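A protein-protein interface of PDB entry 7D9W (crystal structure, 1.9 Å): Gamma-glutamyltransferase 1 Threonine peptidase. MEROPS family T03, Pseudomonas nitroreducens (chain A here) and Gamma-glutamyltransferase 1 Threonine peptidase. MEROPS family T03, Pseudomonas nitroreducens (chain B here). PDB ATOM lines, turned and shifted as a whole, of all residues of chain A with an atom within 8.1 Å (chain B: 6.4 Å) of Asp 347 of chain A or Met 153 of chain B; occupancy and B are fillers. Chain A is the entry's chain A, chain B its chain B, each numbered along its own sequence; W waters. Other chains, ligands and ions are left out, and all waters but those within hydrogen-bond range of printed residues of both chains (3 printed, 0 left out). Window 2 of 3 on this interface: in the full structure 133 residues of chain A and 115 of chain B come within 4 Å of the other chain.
A ring nitrogen (ND1) of His 301 of chain A is in hydrogen-bond range of the side-chain hydroxyl (OH) of Tyr 155 of chain B (2.8 Å).
Water W3 lies within hydrogen-bond range of OE1 of Glu 149 of chain B (2.6 Å) and N of Ala 297 of chain A (2.8 Å).
Water W2 bridges the side-chain carboxylate of Glu 305 of chain A (2.7 Å) and the side-chain hydroxyl of Tyr 155 of chain B (2.8 Å).
Water W1 bridges O of Met 153 of chain B (2.7 Å) and N of Ile 349 of chain A (3.1 Å).
OE1 of Glu 149 of chain B touches CB of Ala 297 of chain A, 3.5 Å away.
Ala 297 of chain A touches Leu 150 of chain B (O to CD2, 3.5 Å).
Leu 150 of chain B touches Ile 300 of chain A (CD1 to CG2, 3.8 Å).
Met 153 of chain B touches His 301 of chain A (CE to CG, 3.2 Å).
Met 153 of chain B touches Asp 347 of chain A.
Ile 349 of chain A touches Met 153 of chain B (CD1 to O, 3.3 Å).
Gly 154 of chain B touches Ile 349 of chain A.
CZ of Tyr 155 of chain B touches CG1 of Ile 349 of chain A (3.6 Å).
Printed residues of chain B within 4 Å of Ala 297 of chain A: Glu 149 (3.5 Å) and Leu 150 (3.5 Å).
Of the printed residues of chain B, Ile 300 of chain A touches Leu 150.
Asp 347 of chain A touches one residue of chain B.
Printed residues of chain B within 4 Å of Ile 349 of chain A: Met 153 (3.3 Å), Gly 154 (3.8 Å) and Tyr 155 (3.6 Å).
No residue of chain A comes within 4 Å of Ala 152 of chain B.
The nearest printed residue of chain B that does not touch Asp 347 of chain A is Tyr 155 of chain B (8.1 Å).
The nearest printed residue of chain A that does not touch Gly 154 of chain B is Ala 348 of chain A (8.1 Å).
O of Asn 345 of chain A is in hydrogen-bond range of NE2 of His 301 of chain A, 2.7 Å away.
The backbone carbonyl oxygen of Ala 348 of chain A lies close to a ring nitrogen (NE2) of His 301 of chain A.
The side-chain amide oxygen (OD1) of Asn 345 of chain A is in hydrogen-bond range of the backbone NH (N) of Asp 347 of chain A (3.0 Å).
The backbone carbonyl oxygen of Leu 150 of chain B lies within hydrogen-bond range of the backbone NH of Tyr 155 of chain B (3.2 Å).
Of the 8 printed residues of chain B, 5 touch a printed residue of chain A.
Printed residues of chain B that touch a printed residue of chain A: Glu 149, Leu 150, Met 153, Gly 154 and Tyr 155.
Hydrophobic or aromatic side chains of chain B that line the printed part of chain A: Leu 150, Met 153 and Tyr 155.
Among the printed residues, no Asp or Glu carboxylate lies within 4 Å of a Lys or Arg side-chain nitrogen of the other chain.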
ATOM      1  N   ARG A 285     -27.542  -1.485 -14.325  1.00  0.00           N
ATOM      2  CA  ARG A 285     -27.733  -0.710 -15.546  1.00  0.00           C
ATOM      3  C   ARG A 285     -28.397  -1.514 -16.665  1.00  0.00           C
ATOM      4  O   ARG A 285     -28.174  -1.219 -17.848  1.00  0.00           O
ATOM      5  CB  ARG A 285     -26.394  -0.157 -16.038  1.00  0.00           C
ATOM      6  CG  ARG A 285     -25.588   0.626 -15.013  1.00  0.00           C
ATOM      7  CD  ARG A 285     -26.323   1.851 -14.488  1.00  0.00           C
ATOM      8  NE  ARG A 285     -26.836   2.709 -15.554  1.00  0.00           N
ATOM      9  CZ  ARG A 285     -26.823   4.041 -15.529  1.00  0.00           C
ATOM     10  NH1 ARG A 285     -26.311   4.695 -14.494  1.00  0.00           N
ATOM     11  NH2 ARG A 285     -27.326   4.723 -16.547  1.00  0.00           N
ATOM     12  N   ASP A 288     -29.924   0.155 -19.733  1.00  0.00           N
ATOM     13  CA  ASP A 288     -29.042   0.743 -20.730  1.00  0.00           C
ATOM     14  C   ASP A 288     -28.493  -0.294 -21.696  1.00  0.00           C
ATOM     15  O   ASP A 288     -28.049   0.067 -22.790  1.00  0.00           O
ATOM     16  CB  ASP A 288     -27.872   1.454 -20.049  1.00  0.00           C
ATOM     17  CG  ASP A 288     -28.326   2.493 -19.056  1.00  0.00           C
ATOM     18  OD1 ASP A 288     -28.548   3.653 -19.458  1.00  0.00           O
ATOM     19  OD2 ASP A 288     -28.478   2.142 -17.867  1.00  0.00           O
ATOM     20  N   ALA A 297     -20.597   0.047 -30.351  1.00  0.00           N
ATOM     21  CA  ALA A 297     -19.918   1.139 -29.660  1.00  0.00           C
ATOM     22  C   ALA A 297     -20.533   1.375 -28.284  1.00  0.00           C
ATOM     23  O   ALA A 297     -19.811   1.542 -27.293  1.00  0.00           O
ATOM     24  CB  ALA A 297     -19.963   2.413 -30.505  1.00  0.00           C
ATOM     25  N   LYS A 298     -21.869   1.362 -28.197  1.00  0.00           N
ATOM     26  CA  LYS A 298     -22.509   1.581 -26.906  1.00  0.00           C
ATOM     27  C   LYS A 298     -22.158   0.477 -25.914  1.00  0.00           C
ATOM     28  O   LYS A 298     -21.914   0.753 -24.734  1.00  0.00           O
ATOM     29  CB  LYS A 298     -24.029   1.675 -27.050  1.00  0.00           C
ATOM     30  CG  LYS A 298     -24.723   2.079 -25.741  1.00  0.00           C
ATOM     31  CD  LYS A 298     -26.161   2.525 -25.961  1.00  0.00           C
ATOM     32  CE  LYS A 298     -26.793   3.050 -24.674  1.00  0.00           C
ATOM     33  N   ILE A 300     -19.434  -1.391 -25.770  1.00  0.00           N
ATOM     34  CA  ILE A 300     -18.046  -1.266 -25.340  1.00  0.00           C
ATOM     35  C   ILE A 300     -17.870  -0.031 -24.473  1.00  0.00           C
ATOM     36  O   ILE A 300     -17.109  -0.040 -23.502  1.00  0.00           O
ATOM     37  CB  ILE A 300     -17.125  -1.251 -26.573  1.00  0.00           C
ATOM     38  CG1 ILE A 300     -17.047  -2.659 -27.175  1.00  0.00           C
ATOM     39  CG2 ILE A 300     -15.748  -0.753 -26.215  1.00  0.00           C
ATOM     40  CD1 ILE A 300     -16.553  -2.698 -28.603  1.00  0.00           C
ATOM     41  N   HIS A 301     -18.583   1.047 -24.796  1.00  0.00           N
ATOM     42  CA  HIS A 301     -18.557   2.225 -23.936  1.00  0.00           C
ATOM     43  C   HIS A 301     -19.085   1.906 -22.540  1.00  0.00           C
ATOM     44  O   HIS A 301     -18.491   2.309 -21.532  1.00  0.00           O
ATOM     45  CB  HIS A 301     -19.370   3.356 -24.564  1.00  0.00           C
ATOM     46  CG  HIS A 301     -19.668   4.461 -23.607  1.00  0.00           C
ATOM     47  ND1 HIS A 301     -18.683   5.266 -23.077  1.00  0.00           N
ATOM     48  CD2 HIS A 301     -20.832   4.879 -23.060  1.00  0.00           C
ATOM     49  CE1 HIS A 301     -19.231   6.140 -22.254  1.00  0.00           C
ATOM     50  NE2 HIS A 301     -20.534   5.927 -22.224  1.00  0.00           N
ATOM     51  N   LEU A 302     -20.208   1.189 -22.459  1.00  0.00           N
ATOM     52  CA  LEU A 302     -20.785   0.865 -21.156  1.00  0.00           C
ATOM     53  C   LEU A 302     -19.833   0.012 -20.326  1.00  0.00           C
ATOM     54  O   LEU A 302     -19.623   0.272 -19.134  1.00  0.00           O
ATOM     55  CB  LEU A 302     -22.126   0.157 -21.343  1.00  0.00           C
ATOM     56  CG  LEU A 302     -23.293   1.043 -21.783  1.00  0.00           C
ATOM     57  CD1 LEU A 302     -24.484   0.169 -22.157  1.00  0.00           C
ATOM     58  CD2 LEU A 302     -23.677   2.045 -20.698  1.00  0.00           C
ATOM     59  N   GLU A 305     -17.109   2.256 -19.034  1.00  0.00           N
ATOM     60  CA  GLU A 305     -17.544   3.065 -17.900  1.00  0.00           C
ATOM     61  C   GLU A 305     -17.535   2.265 -16.606  1.00  0.00           C
ATOM     62  O   GLU A 305     -17.194   2.794 -15.542  1.00  0.00           O
ATOM     63  CB  GLU A 305     -18.940   3.618 -18.151  1.00  0.00           C
ATOM     64  CG  GLU A 305     -18.978   4.772 -19.115  1.00  0.00           C
ATOM     65  CD  GLU A 305     -18.486   6.055 -18.484  1.00  0.00           C
ATOM     66  OE1 GLU A 305     -19.140   6.532 -17.535  1.00  0.00           O
ATOM     67  OE2 GLU A 305     -17.458   6.589 -18.948  1.00  0.00           O
ATOM     68  N   VAL A 344     -22.209   5.515 -13.780  1.00  0.00           N
ATOM     69  CA  VAL A 344     -22.029   5.164 -15.182  1.00  0.00           C
ATOM     70  C   VAL A 344     -22.742   6.179 -16.060  1.00  0.00           C
ATOM     71  O   VAL A 344     -23.922   6.489 -15.851  1.00  0.00           O
ATOM     72  CB  VAL A 344     -22.544   3.738 -15.436  1.00  0.00           C
ATOM     73  CG1 VAL A 344     -22.685   3.468 -16.923  1.00  0.00           C
ATOM     74  CG2 VAL A 344     -21.615   2.712 -14.779  1.00  0.00           C
ATOM     75  N   ASN A 345     -22.024   6.705 -17.053  1.00  0.00           N
ATOM     76  CA  ASN A 345     -22.613   7.631 -18.006  1.00  0.00           C
ATOM     77  C   ASN A 345     -22.854   6.894 -19.315  1.00  0.00           C
ATOM     78  O   ASN A 345     -21.886   6.591 -20.032  1.00  0.00           O
ATOM     79  CB  ASN A 345     -21.697   8.832 -18.230  1.00  0.00           C
ATOM     80  CG  ASN A 345     -22.349   9.908 -19.070  1.00  0.00           C
ATOM     81  OD1 ASN A 345     -23.247   9.632 -19.867  1.00  0.00           O
ATOM     82  ND2 ASN A 345     -21.897  11.146 -18.901  1.00  0.00           N
ATOM     83  N   PRO A 346     -24.101   6.572 -19.670  1.00  0.00           N
ATOM     84  CA  PRO A 346     -24.330   5.770 -20.878  1.00  0.00           C
ATOM     85  C   PRO A 346     -24.162   6.540 -22.174  1.00  0.00           C
ATOM     86  O   PRO A 346     -24.161   5.918 -23.245  1.00  0.00           O
ATOM     87  CB  PRO A 346     -25.786   5.299 -20.720  1.00  0.00           C
ATOM     88  CG  PRO A 346     -26.425   6.319 -19.862  1.00  0.00           C
ATOM     89  CD  PRO A 346     -25.358   6.898 -18.966  1.00  0.00           C
ATOM     90  N   ASP A 347     -24.010   7.861 -22.113  1.00  0.00           N
ATOM     91  CA  ASP A 347     -24.008   8.688 -23.311  1.00  0.00           C
ATOM     92  C   ASP A 347     -22.661   9.317 -23.627  1.00  0.00           C
ATOM     93  O   ASP A 347     -22.436   9.696 -24.779  1.00  0.00           O
ATOM     94  CB  ASP A 347     -25.058   9.801 -23.170  1.00  0.00           C
ATOM     95  CG  ASP A 347     -26.457   9.252 -22.981  1.00  0.00           C
ATOM     96  OD1 ASP A 347     -26.852   8.355 -23.756  1.00  0.00           O
ATOM     97  OD2 ASP A 347     -27.160   9.699 -22.050  1.00  0.00           O
ATOM     98  N   ALA A 348     -21.762   9.418 -22.654  1.00  0.00           N
ATOM     99  CA  ALA A 348     -20.494  10.101 -22.857  1.00  0.00           C
ATOM    100  C   ALA A 348     -19.466   9.527 -21.896  1.00  0.00           C
ATOM    101  O   ALA A 348     -19.810   8.871 -20.910  1.00  0.00           O
ATOM    102  CB  ALA A 348     -20.640  11.614 -22.647  1.00  0.00           C
ATOM    103  N   ILE A 349     -18.192   9.783 -22.189  1.00  0.00           N
ATOM    104  CA  ILE A 349     -17.132   9.304 -21.314  1.00  0.00           C
ATOM    105  C   ILE A 349     -17.125  10.127 -20.033  1.00  0.00           C
ATOM    106  O   ILE A 349     -17.203  11.361 -20.066  1.00  0.00           O
ATOM    107  CB  ILE A 349     -15.769   9.365 -22.023  1.00  0.00           C
ATOM    108  CG1 ILE A 349     -15.767   8.463 -23.260  1.00  0.00           C
ATOM    109  CG2 ILE A 349     -14.652   8.977 -21.064  1.00  0.00           C
ATOM    110  CD1 ILE A 349     -14.519   8.598 -24.116  1.00  0.00           C
ATOM    111  N   SER A 350     -17.036   9.443 -18.895  1.00  0.00           N
ATOM    112  CA  SER A 350     -16.872  10.133 -17.625  1.00  0.00           C
ATOM    113  C   SER A 350     -15.490  10.766 -17.549  1.00  0.00           C
ATOM    114  O   SER A 350     -14.497  10.178 -17.983  1.00  0.00           O
ATOM    115  CB  SER A 350     -17.053   9.164 -16.459  1.00  0.00           C
ATOM    116  OG  SER A 350     -18.403   8.762 -16.316  1.00  0.00           O
ATOM    117  N   ASP B 148     -14.571   3.905 -35.318  1.00  0.00           N
ATOM    118  CA  ASP B 148     -14.798   5.321 -35.582  1.00  0.00           C
ATOM    119  C   ASP B 148     -15.707   5.935 -34.526  1.00  0.00           C
ATOM    120  O   ASP B 148     -15.476   7.060 -34.069  1.00  0.00           O
ATOM    121  CB  ASP B 148     -15.413   5.499 -36.970  1.00  0.00           C
ATOM    122  CG  ASP B 148     -14.392   5.384 -38.078  1.00  0.00           C
ATOM    123  OD1 ASP B 148     -13.186   5.538 -37.790  1.00  0.00           O
ATOM    124  OD2 ASP B 148     -14.792   5.131 -39.232  1.00  0.00           O
ATOM    125  N   GLU B 149     -16.751   5.204 -34.129  1.00  0.00           N
ATOM    126  CA  GLU B 149     -17.714   5.747 -33.179  1.00  0.00           C
ATOM    127  C   GLU B 149     -17.105   5.883 -31.789  1.00  0.00           C
ATOM    128  O   GLU B 149     -17.365   6.868 -31.090  1.00  0.00           O
ATOM    129  CB  GLU B 149     -18.964   4.863 -33.151  1.00  0.00           C
ATOM    130  CG  GLU B 149     -19.892   5.124 -34.338  1.00  0.00           C
ATOM    131  CD  GLU B 149     -20.985   4.082 -34.509  1.00  0.00           C
ATOM    132  OE1 GLU B 149     -21.031   3.119 -33.720  1.00  0.00           O
ATOM    133  OE2 GLU B 149     -21.795   4.225 -35.451  1.00  0.00           O
ATOM    134  N   LEU B 150     -16.293   4.911 -31.371  1.00  0.00           N
ATOM    135  CA  LEU B 150     -15.621   5.022 -30.080  1.00  0.00           C
ATOM    136  C   LEU B 150     -14.589   6.144 -30.092  1.00  0.00           C
ATOM    137  O   LEU B 150     -14.447   6.877 -29.107  1.00  0.00           O
ATOM    138  CB  LEU B 150     -14.957   3.695 -29.714  1.00  0.00           C
ATOM    139  CG  LEU B 150     -15.858   2.490 -29.440  1.00  0.00           C
ATOM    140  CD1 LEU B 150     -15.036   1.200 -29.375  1.00  0.00           C
ATOM    141  CD2 LEU B 150     -16.644   2.698 -28.155  1.00  0.00           C
ATOM    142  N   LYS B 151     -13.838   6.277 -31.187  1.00  0.00           N
ATOM    143  CA  LYS B 151     -12.892   7.381 -31.294  1.00  0.00           C
ATOM    144  C   LYS B 151     -13.616   8.725 -31.282  1.00  0.00           C
ATOM    145  O   LYS B 151     -13.109   9.705 -30.724  1.00  0.00           O
ATOM    146  CB  LYS B 151     -12.054   7.239 -32.566  1.00  0.00           C
ATOM    147  CG  LYS B 151     -11.067   6.062 -32.586  1.00  0.00           C
ATOM    148  CD  LYS B 151     -10.450   5.924 -33.982  1.00  0.00           C
ATOM    149  CE  LYS B 151      -9.048   5.331 -33.972  1.00  0.00           C
ATOM    150  NZ  LYS B 151      -8.775   4.585 -35.239  1.00  0.00           N
ATOM    151  N   ALA B 152     -14.801   8.793 -31.895  1.00  0.00           N
ATOM    152  CA  ALA B 152     -15.543  10.050 -31.899  1.00  0.00           C
ATOM    153  C   ALA B 152     -15.944  10.458 -30.488  1.00  0.00           C
ATOM    154  O   ALA B 152     -16.085  11.654 -30.203  1.00  0.00           O
ATOM    155  CB  ALA B 152     -16.784   9.940 -32.787  1.00  0.00           C
ATOM    156  N   MET B 153     -16.144   9.480 -29.599  1.00  0.00           N
ATOM    157  CA  MET B 153     -16.476   9.781 -28.217  1.00  0.00           C
ATOM    158  C   MET B 153     -15.281  10.284 -27.429  1.00  0.00           C
ATOM    159  O   MET B 153     -15.461  10.817 -26.328  1.00  0.00           O
ATOM    160  CB  MET B 153     -17.001   8.549 -27.493  1.00  0.00           C
ATOM    161  CG  MET B 153     -18.450   8.246 -27.712  1.00  0.00           C
ATOM    162  SD  MET B 153     -18.820   6.594 -27.101  1.00  0.00           S
ATOM    163  CE  MET B 153     -19.725   7.005 -25.613  1.00  0.00           C
ATOM    164  N   GLY B 154     -14.071  10.052 -27.930  1.00  0.00           N
ATOM    165  CA  GLY B 154     -12.868  10.478 -27.252  1.00  0.00           C
ATOM    166  C   GLY B 154     -11.959   9.360 -26.784  1.00  0.00           C
ATOM    167  O   GLY B 154     -10.987   9.631 -26.070  1.00  0.00           O
ATOM    168  N   TYR B 155     -12.239   8.114 -27.167  1.00  0.00           N
ATOM    169  CA  TYR B 155     -11.379   7.002 -26.783  1.00  0.00           C
ATOM    170  C   TYR B 155     -10.165   6.896 -27.699  1.00  0.00           C
ATOM    171  O   TYR B 155     -10.241   7.165 -28.900  1.00  0.00           O
ATOM    172  CB  TYR B 155     -12.118   5.663 -26.842  1.00  0.00           C
ATOM    173  CG  TYR B 155     -13.135   5.438 -25.757  1.00  0.00           C
ATOM    174  CD1 TYR B 155     -12.743   5.253 -24.439  1.00  0.00           C
ATOM    175  CD2 TYR B 155     -14.489   5.397 -26.050  1.00  0.00           C
ATOM    176  CE1 TYR B 155     -13.675   5.041 -23.442  1.00  0.00           C
ATOM    177  CE2 TYR B 155     -15.428   5.183 -25.059  1.00  0.00           C
ATOM    178  CZ  TYR B 155     -15.015   4.999 -23.758  1.00  0.00           C
ATOM    179  OH  TYR B 155     -15.948   4.789 -22.764  1.00  0.00           O
HETATM  180  O   HOH W   1     -17.721  11.251 -24.828  1.00  0.00           O
HETATM  181  O   HOH W   2     -15.430   5.260 -20.048  1.00  0.00           O
HETATM  182  O   HOH W   3     -21.822   0.802 -32.808  1.00  0.00           O
